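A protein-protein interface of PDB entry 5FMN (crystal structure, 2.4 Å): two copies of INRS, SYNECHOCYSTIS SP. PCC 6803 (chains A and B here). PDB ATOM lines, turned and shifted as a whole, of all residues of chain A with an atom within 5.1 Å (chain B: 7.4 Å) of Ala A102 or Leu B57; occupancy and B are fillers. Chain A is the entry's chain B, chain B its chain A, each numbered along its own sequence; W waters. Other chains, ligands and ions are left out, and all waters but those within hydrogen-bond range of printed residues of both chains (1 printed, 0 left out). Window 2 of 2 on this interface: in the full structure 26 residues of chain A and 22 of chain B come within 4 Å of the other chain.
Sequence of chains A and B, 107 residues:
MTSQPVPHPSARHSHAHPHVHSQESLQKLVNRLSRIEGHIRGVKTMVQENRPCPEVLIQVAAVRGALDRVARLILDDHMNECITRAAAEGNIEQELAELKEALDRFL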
ATOM      1  N   ALA A  71      10.063  -9.081  33.440  1.00  0.00           N
ATOM      2  CA  ALA A  71      11.490  -9.181  33.285  1.00  0.00           C
ATOM      3  C   ALA A  71      12.134  -9.245  34.647  1.00  0.00           C
ATOM      4  O   ALA A  71      12.990 -10.088  34.899  1.00  0.00           O
ATOM      5  CB  ALA A  71      12.022  -8.000  32.482  1.00  0.00           C
ATOM      6  N   ILE A  74      11.897 -12.592  36.364  1.00  0.00           N
ATOM      7  CA  ILE A  74      12.746 -13.621  35.753  1.00  0.00           C
ATOM      8  C   ILE A  74      14.192 -13.448  36.193  1.00  0.00           C
ATOM      9  O   ILE A  74      14.897 -14.425  36.488  1.00  0.00           O
ATOM     10  CB  ILE A  74      12.694 -13.550  34.202  1.00  0.00           C
ATOM     11  CG1 ILE A  74      11.306 -13.963  33.702  1.00  0.00           C
ATOM     12  CG2 ILE A  74      13.757 -14.457  33.589  1.00  0.00           C
ATOM     13  CD1 ILE A  74      10.990 -13.507  32.296  1.00  0.00           C
ATOM     14  N   LEU A  75      14.606 -12.185  36.244  1.00  0.00           N
ATOM     15  CA  LEU A  75      15.894 -11.823  36.764  1.00  0.00           C
ATOM     16  C   LEU A  75      16.109 -12.167  38.241  1.00  0.00           C
ATOM     17  O   LEU A  75      17.183 -12.636  38.617  1.00  0.00           O
ATOM     18  CB  LEU A  75      16.139 -10.337  36.533  1.00  0.00           C
ATOM     19  CG  LEU A  75      17.495  -9.792  36.975  1.00  0.00           C
ATOM     20  CD1 LEU A  75      18.586 -10.340  36.067  1.00  0.00           C
ATOM     21  CD2 LEU A  75      17.490  -8.270  36.967  1.00  0.00           C
ATOM     22  N   HIS A  78      16.729 -15.906  38.473  1.00  0.00           N
ATOM     23  CA  HIS A  78      18.090 -16.140  37.999  1.00  0.00           C
ATOM     24  C   HIS A  78      19.165 -15.787  39.051  1.00  0.00           C
ATOM     25  O   HIS A  78      20.027 -16.606  39.374  1.00  0.00           O
ATOM     26  CB  HIS A  78      18.323 -15.355  36.717  1.00  0.00           C
ATOM     27  CG  HIS A  78      19.631 -15.664  36.049  1.00  0.00           C
ATOM     28  ND1 HIS A  78      19.838 -16.801  35.298  1.00  0.00           N
ATOM     29  CD2 HIS A  78      20.800 -14.979  36.027  1.00  0.00           C
ATOM     30  CE1 HIS A  78      21.088 -16.819  34.872  1.00  0.00           C
ATOM     31  NE2 HIS A  78      21.702 -15.741  35.329  1.00  0.00           N
ATOM     32  N   GLU A  98      27.660 -15.130  35.057  1.00  0.00           N
ATOM     33  CA  GLU A  98      26.270 -15.458  34.737  1.00  0.00           C
ATOM     34  C   GLU A  98      25.292 -14.344  35.094  1.00  0.00           C
ATOM     35  O   GLU A  98      24.304 -14.099  34.394  1.00  0.00           O
ATOM     36  CB  GLU A  98      25.837 -16.701  35.517  1.00  0.00           C
ATOM     37  CG  GLU A  98      26.124 -17.997  34.794  1.00  0.00           C
ATOM     38  CD  GLU A  98      25.015 -18.348  33.843  1.00  0.00           C
ATOM     39  OE1 GLU A  98      23.914 -18.701  34.319  1.00  0.00           O
ATOM     40  OE2 GLU A  98      25.227 -18.186  32.624  1.00  0.00           O
ATOM     41  N   LEU A  99      25.513 -13.736  36.248  1.00  0.00           N
ATOM     42  CA  LEU A  99      24.624 -12.701  36.693  1.00  0.00           C
ATOM     43  C   LEU A  99      24.779 -11.544  35.748  1.00  0.00           C
ATOM     44  O   LEU A  99      23.785 -10.934  35.374  1.00  0.00           O
ATOM     45  CB  LEU A  99      24.959 -12.225  38.106  1.00  0.00           C
ATOM     46  CG  LEU A  99      23.723 -11.914  38.942  1.00  0.00           C
ATOM     47  CD1 LEU A  99      24.134 -11.395  40.310  1.00  0.00           C
ATOM     48  CD2 LEU A  99      22.826 -10.909  38.231  1.00  0.00           C
ATOM     49  N   LYS A 100      26.029 -11.212  35.411  1.00  0.00           N
ATOM     50  CA  LYS A 100      26.328  -9.994  34.657  1.00  0.00           C
ATOM     51  C   LYS A 100      25.780 -10.062  33.245  1.00  0.00           C
ATOM     52  O   LYS A 100      25.298  -9.052  32.750  1.00  0.00           O
ATOM     53  CB  LYS A 100      27.824  -9.693  34.642  1.00  0.00           C
ATOM     54  CG  LYS A 100      28.329  -9.165  35.980  1.00  0.00           C
ATOM     55  CD  LYS A 100      29.811  -9.414  36.205  1.00  0.00           C
ATOM     56  CE  LYS A 100      30.306  -8.650  37.420  1.00  0.00           C
ATOM     57  NZ  LYS A 100      31.785  -8.509  37.392  1.00  0.00           N
ATOM     58  N   GLU A 101      25.792 -11.260  32.650  1.00  0.00           N
ATOM     59  CA  GLU A 101      25.202 -11.475  31.347  1.00  0.00           C
ATOM     60  C   GLU A 101      23.717 -11.186  31.379  1.00  0.00           C
ATOM     61  O   GLU A 101      23.161 -10.639  30.426  1.00  0.00           O
ATOM     62  CB  GLU A 101      25.371 -12.930  30.824  1.00  0.00           C
ATOM     63  CG  GLU A 101      25.495 -12.951  29.280  1.00  0.00           C
ATOM     64  CD  GLU A 101      24.929 -14.187  28.540  1.00  0.00           C
ATOM     65  OE1 GLU A 101      25.214 -15.361  28.900  1.00  0.00           O
ATOM     66  OE2 GLU A 101      24.262 -13.978  27.491  1.00  0.00           O
ATOM     67  N   ALA A 102      23.065 -11.693  32.415  1.00  0.00           N
ATOM     68  CA  ALA A 102      21.642 -11.532  32.560  1.00  0.00           C
ATOM     69  C   ALA A 102      21.289 -10.059  32.746  1.00  0.00           C
ATOM     70  O   ALA A 102      20.319  -9.590  32.164  1.00  0.00           O
ATOM     71  CB  ALA A 102      21.155 -12.355  33.734  1.00  0.00           C
ATOM     72  N   LEU A 103      22.053  -9.338  33.566  1.00  0.00           N
ATOM     73  CA  LEU A 103      21.905  -7.874  33.696  1.00  0.00           C
ATOM     74  C   LEU A 103      22.215  -7.106  32.432  1.00  0.00           C
ATOM     75  O   LEU A 103      21.629  -6.069  32.173  1.00  0.00           O
ATOM     76  CB  LEU A 103      22.836  -7.321  34.783  1.00  0.00           C
ATOM     77  CG  LEU A 103      22.425  -7.480  36.225  1.00  0.00           C
ATOM     78  CD1 LEU A 103      23.508  -6.944  37.138  1.00  0.00           C
ATOM     79  CD2 LEU A 103      21.123  -6.732  36.451  1.00  0.00           C
ATOM     80  N   ASP A 104      23.218  -7.540  31.686  1.00  0.00           N
ATOM     81  CA  ASP A 104      23.500  -6.883  30.412  1.00  0.00           C
ATOM     82  C   ASP A 104      22.222  -6.875  29.588  1.00  0.00           C
ATOM     83  O   ASP A 104      21.802  -5.820  29.138  1.00  0.00           O
ATOM     84  CB  ASP A 104      24.635  -7.589  29.671  1.00  0.00           C
ATOM     85  CG  ASP A 104      26.011  -7.361  30.333  1.00  0.00           C
ATOM     86  OD1 ASP A 104      26.175  -6.362  31.076  1.00  0.00           O
ATOM     87  OD2 ASP A 104      26.945  -8.168  30.066  1.00  0.00           O
ATOM     88  N   ARG A 105      21.569  -8.035  29.447  1.00  0.00           N
ATOM     89  CA  ARG A 105      20.431  -8.169  28.503  1.00  0.00           C
ATOM     90  C   ARG A 105      19.142  -7.611  29.099  1.00  0.00           C
ATOM     91  O   ARG A 105      18.210  -7.289  28.377  1.00  0.00           O
ATOM     92  CB  ARG A 105      20.228  -9.632  28.016  1.00  0.00           C
ATOM     93  CG  ARG A 105      21.501 -10.333  27.478  1.00  0.00           C
ATOM     94  CD  ARG A 105      21.916 -10.048  26.034  1.00  0.00           C
ATOM     95  NE  ARG A 105      22.681  -8.805  25.912  1.00  0.00           N
ATOM     96  CZ  ARG A 105      23.954  -8.635  26.315  1.00  0.00           C
ATOM     97  NH1 ARG A 105      24.634  -9.615  26.928  1.00  0.00           N
ATOM     98  NH2 ARG A 105      24.538  -7.444  26.148  1.00  0.00           N
ATOM     99  N   PHE A 106      19.113  -7.470  30.419  1.00  0.00           N
ATOM    100  CA  PHE A 106      18.012  -6.808  31.126  1.00  0.00           C
ATOM    101  C   PHE A 106      18.039  -5.275  31.045  1.00  0.00           C
ATOM    102  O   PHE A 106      16.992  -4.657  31.109  1.00  0.00           O
ATOM    103  CB  PHE A 106      18.026  -7.226  32.602  1.00  0.00           C
ATOM    104  CG  PHE A 106      16.880  -6.690  33.397  1.00  0.00           C
ATOM    105  CD1 PHE A 106      16.961  -5.441  34.008  1.00  0.00           C
ATOM    106  CD2 PHE A 106      15.725  -7.439  33.563  1.00  0.00           C
ATOM    107  CE1 PHE A 106      15.900  -4.943  34.751  1.00  0.00           C
ATOM    108  CE2 PHE A 106      14.662  -6.938  34.293  1.00  0.00           C
ATOM    109  CZ  PHE A 106      14.744  -5.691  34.885  1.00  0.00           C
ATOM    110  N   VAL B  43       7.859 -15.232  23.426  1.00  0.00           N
ATOM    111  CA  VAL B  43       8.416 -15.252  24.775  1.00  0.00           C
ATOM    112  C   VAL B  43       7.728 -16.259  25.707  1.00  0.00           C
ATOM    113  O   VAL B  43       8.416 -16.895  26.513  1.00  0.00           O
ATOM    114  CB  VAL B  43       8.345 -13.859  25.434  1.00  0.00           C
ATOM    115  CG1 VAL B  43       8.912 -13.877  26.845  1.00  0.00           C
ATOM    116  CG2 VAL B  43       9.118 -12.855  24.590  1.00  0.00           C
ATOM    117  N   MET B  46       8.822 -19.728  24.875  1.00  0.00           N
ATOM    118  CA  MET B  46      10.205 -19.935  25.332  1.00  0.00           C
ATOM    119  C   MET B  46      10.260 -20.322  26.812  1.00  0.00           C
ATOM    120  O   MET B  46      11.127 -21.051  27.239  1.00  0.00           O
ATOM    121  CB  MET B  46      11.056 -18.677  25.134  1.00  0.00           C
ATOM    122  CG  MET B  46      11.494 -18.422  23.700  1.00  0.00           C
ATOM    123  SD  MET B  46      12.594 -16.992  23.519  1.00  0.00           S
ATOM    124  CE  MET B  46      14.001 -17.500  24.472  1.00  0.00           C
ATOM    125  N   PRO B  52      17.146 -20.923  28.301  1.00  0.00           N
ATOM    126  CA  PRO B  52      17.929 -20.148  29.268  1.00  0.00           C
ATOM    127  C   PRO B  52      17.448 -18.690  29.464  1.00  0.00           C
ATOM    128  O   PRO B  52      16.946 -18.047  28.546  1.00  0.00           O
ATOM    129  CB  PRO B  52      19.341 -20.134  28.674  1.00  0.00           C
ATOM    130  CG  PRO B  52      19.358 -21.229  27.667  1.00  0.00           C
ATOM    131  CD  PRO B  52      17.960 -21.345  27.147  1.00  0.00           C
ATOM    132  N   CYS B  53      17.726 -18.158  30.638  1.00  0.00           N
ATOM    133  CA  CYS B  53      17.290 -16.836  31.022  1.00  0.00           C
ATOM    134  C   CYS B  53      17.760 -15.719  30.067  1.00  0.00           C
ATOM    135  O   CYS B  53      16.958 -14.873  29.682  1.00  0.00           O
ATOM    136  CB  CYS B  53      17.745 -16.602  32.486  1.00  0.00           C
ATOM    137  SG  CYS B  53      17.537 -14.970  33.240  1.00  0.00           S
ATOM    138  N   PRO B  54      19.055 -15.682  29.726  1.00  0.00           N
ATOM    139  CA  PRO B  54      19.544 -14.647  28.792  1.00  0.00           C
ATOM    140  C   PRO B  54      18.845 -14.626  27.432  1.00  0.00           C
ATOM    141  O   PRO B  54      18.625 -13.546  26.894  1.00  0.00           O
ATOM    142  CB  PRO B  54      21.030 -14.994  28.618  1.00  0.00           C
ATOM    143  CG  PRO B  54      21.404 -15.718  29.883  1.00  0.00           C
ATOM    144  CD  PRO B  54      20.163 -16.421  30.364  1.00  0.00           C
ATOM    145  N   GLU B  55      18.561 -15.806  26.878  1.00  0.00           N
ATOM    146  CA  GLU B  55      17.774 -15.929  25.629  1.00  0.00           C
ATOM    147  C   GLU B  55      16.372 -15.366  25.756  1.00  0.00           C
ATOM    148  O   GLU B  55      15.921 -14.665  24.852  1.00  0.00           O
ATOM    149  CB  GLU B  55      17.637 -17.380  25.142  1.00  0.00           C
ATOM    150  CG  GLU B  55      18.932 -17.993  24.620  1.00  0.00           C
ATOM    151  CD  GLU B  55      18.732 -19.376  24.004  1.00  0.00           C
ATOM    152  OE1 GLU B  55      17.539 -19.812  23.855  1.00  0.00           O
ATOM    153  OE2 GLU B  55      19.785 -20.016  23.719  1.00  0.00           O
ATOM    154  N   VAL B  56      15.719 -15.649  26.882  1.00  0.00           N
ATOM    155  CA  VAL B  56      14.386 -15.118  27.162  1.00  0.00           C
ATOM    156  C   VAL B  56      14.449 -13.612  27.305  1.00  0.00           C
ATOM    157  O   VAL B  56      13.690 -12.902  26.643  1.00  0.00           O
ATOM    158  CB  VAL B  56      13.758 -15.770  28.418  1.00  0.00           C
ATOM    159  CG1 VAL B  56      12.436 -15.112  28.767  1.00  0.00           C
ATOM    160  CG2 VAL B  56      13.515 -17.266  28.176  1.00  0.00           C
ATOM    161  N   LEU B  57      15.445 -13.118  28.041  1.00  0.00           N
ATOM    162  CA  LEU B  57      15.617 -11.655  28.205  1.00  0.00           C
ATOM    163  C   LEU B  57      15.987 -10.905  26.923  1.00  0.00           C
ATOM    164  O   LEU B  57      15.573  -9.759  26.753  1.00  0.00           O
ATOM    165  CB  LEU B  57      16.637 -11.344  29.288  1.00  0.00           C
ATOM    166  CG  LEU B  57      16.222 -11.773  30.703  1.00  0.00           C
ATOM    167  CD1 LEU B  57      17.348 -11.521  31.687  1.00  0.00           C
ATOM    168  CD2 LEU B  57      14.960 -11.046  31.171  1.00  0.00           C
ATOM    169  N   ILE B  58      16.763 -11.548  26.037  1.00  0.00           N
ATOM    170  CA  ILE B  58      17.041 -11.023  24.692  1.00  0.00           C
ATOM    171  C   ILE B  58      15.778 -10.811  23.854  1.00  0.00           C
ATOM    172  O   ILE B  58      15.613  -9.781  23.198  1.00  0.00           O
ATOM    173  CB  ILE B  58      18.011 -11.942  23.918  1.00  0.00           C
ATOM    174  CG1 ILE B  58      19.467 -11.689  24.358  1.00  0.00           C
ATOM    175  CG2 ILE B  58      17.900 -11.729  22.413  1.00  0.00           C
ATOM    176  CD1 ILE B  58      20.348 -12.910  24.316  1.00  0.00           C
ATOM    177  N   GLN B  59      14.845 -11.742  23.967  1.00  0.00           N
ATOM    178  CA  GLN B  59      13.540 -11.643  23.304  1.00  0.00           C
ATOM    179  C   GLN B  59      12.602 -10.575  23.954  1.00  0.00           C
ATOM    180  O   GLN B  59      11.946  -9.788  23.269  1.00  0.00           O
ATOM    181  CB  GLN B  59      12.897 -13.051  23.291  1.00  0.00           C
ATOM    182  CG  GLN B  59      12.210 -13.422  21.987  1.00  0.00           C
ATOM    183  CD  GLN B  59      13.140 -13.330  20.766  1.00  0.00           C
ATOM    184  OE1 GLN B  59      12.897 -12.474  19.953  1.00  0.00           O
ATOM    185  NE2 GLN B  59      14.238 -14.152  20.663  1.00  0.00           N
ATOM    186  N   VAL B  60      12.601 -10.518  25.275  1.00  0.00           N
ATOM    187  CA  VAL B  60      11.903  -9.462  26.043  1.00  0.00           C
ATOM    188  C   VAL B  60      12.436  -8.061  25.708  1.00  0.00           C
ATOM    189  O   VAL B  60      11.645  -7.132  25.607  1.00  0.00           O
ATOM    190  CB  VAL B  60      12.087  -9.700  27.570  1.00  0.00           C
ATOM    191  CG1 VAL B  60      11.563  -8.536  28.393  1.00  0.00           C
ATOM    192  CG2 VAL B  60      11.406 -11.004  28.017  1.00  0.00           C
ATOM    193  N   ALA B  61      13.760  -7.920  25.521  1.00  0.00           N
ATOM    194  CA  ALA B  61      14.382  -6.632  25.134  1.00  0.00           C
ATOM    195  C   ALA B  61      13.889  -6.174  23.767  1.00  0.00           C
ATOM    196  O   ALA B  61      13.543  -5.005  23.569  1.00  0.00           O
ATOM    197  CB  ALA B  61      15.912  -6.757  25.125  1.00  0.00           C
ATOM    198  N   ALA B  62      13.738  -7.122  22.857  1.00  0.00           N
ATOM    199  CA  ALA B  62      13.285  -6.811  21.509  1.00  0.00           C
ATOM    200  C   ALA B  62      11.833  -6.369  21.548  1.00  0.00           C
ATOM    201  O   ALA B  62      11.431  -5.484  20.790  1.00  0.00           O
ATOM    202  CB  ALA B  62      13.430  -8.045  20.637  1.00  0.00           C
ATOM    203  N   VAL B  63      11.024  -7.037  22.377  1.00  0.00           N
ATOM    204  CA  VAL B  63       9.618  -6.655  22.561  1.00  0.00           C
ATOM    205  C   VAL B  63       9.560  -5.239  23.158  1.00  0.00           C
ATOM    206  O   VAL B  63       8.757  -4.389  22.736  1.00  0.00           O
ATOM    207  CB  VAL B  63       8.881  -7.611  23.529  1.00  0.00           C
ATOM    208  CG1 VAL B  63       7.499  -7.096  23.872  1.00  0.00           C
ATOM    209  CG2 VAL B  63       8.779  -9.005  22.955  1.00  0.00           C
ATOM    210  N   ARG B  64      10.410  -4.976  24.138  1.00  0.00           N
ATOM    211  CA  ARG B  64      10.420  -3.640  24.730  1.00  0.00           C
ATOM    212  C   ARG B  64      10.859  -2.573  23.728  1.00  0.00           C
ATOM    213  O   ARG B  64      10.249  -1.523  23.610  1.00  0.00           O
ATOM    214  CB  ARG B  64      11.276  -3.625  25.960  1.00  0.00           C
ATOM    215  CG  ARG B  64      11.608  -2.234  26.419  1.00  0.00           C
ATOM    216  CD  ARG B  64      11.939  -2.281  27.902  1.00  0.00           C
ATOM    217  NE  ARG B  64      12.976  -3.288  28.130  1.00  0.00           N
ATOM    218  CZ  ARG B  64      12.880  -4.341  28.944  1.00  0.00           C
ATOM    219  NH1 ARG B  64      11.814  -4.530  29.715  1.00  0.00           N
ATOM    220  NH2 ARG B  64      13.881  -5.215  28.988  1.00  0.00           N
HETATM  221  O   HOH W   1      15.472  -7.583  28.516  1.00  0.00           O
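SG of Cys B53 lies close to ND1 of His A78 (3.6 Å).
NE2 of His A78 lies within hydrogen-bond range of O of Glu A98 (3.2 Å).
Among the printed residues, merely in contact across the chains: Arg A105 with Ile B58 (3.4 Å), Glu A101 with Pro B54 (3.6 Å), Ala A102 with Leu B57 (3.6 Å), Phe A106 with Arg B64 (3.8 Å), Ile A74 with Cys B53 (3.8 Å) and Arg A105 with Leu B57 (3.96 Å).
Leu B57 touches just these residues of chain A: Ala A102 (3.6 Å) and Arg A105 (3.96 Å).
Printed residues of chain B within 4 Å of Phe A106: Arg B64 (3.8 Å).
Printed residues of chain B within 4 Å of His A78: Cys B53 (3.5 Å).
Of the printed residues of chain B, Glu A101 touches Pro B54.
Of the printed residues of chain A, Cys B53 touches Ile A74 (3.8 Å) and His A78 (3.5 Å).
The nearest residue of chain B that does not touch Ala A102 is Cys B53 (4.5 Å).
The nearest printed residue of chain A that does not touch Ile B58 is Glu A101 (5.2 Å).
Of the 13 printed residues of chain A, 6 touch a printed residue of chain B.
Hydrophobic or aromatic side chains of chain A within 4 Å of the printed part of chain B: Ile A74 and His A78.
Printed residues of chain B that touch a printed residue of chain A: Cys B53, Pro B54, Leu B57, Ile B58 and Arg B64.
No position is printed for both chains.
Of the 7 pairs that touch across the chains among the printed residues, none has its exchanged pair printed and touching as well.
Water W1 lies within hydrogen-bond range of O of Arg A105 (2.8 Å), O of Leu B57 (2.8 Å), NH2 of Arg B64 (2.9 Å) and N of Ala B61 (3.5 Å).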
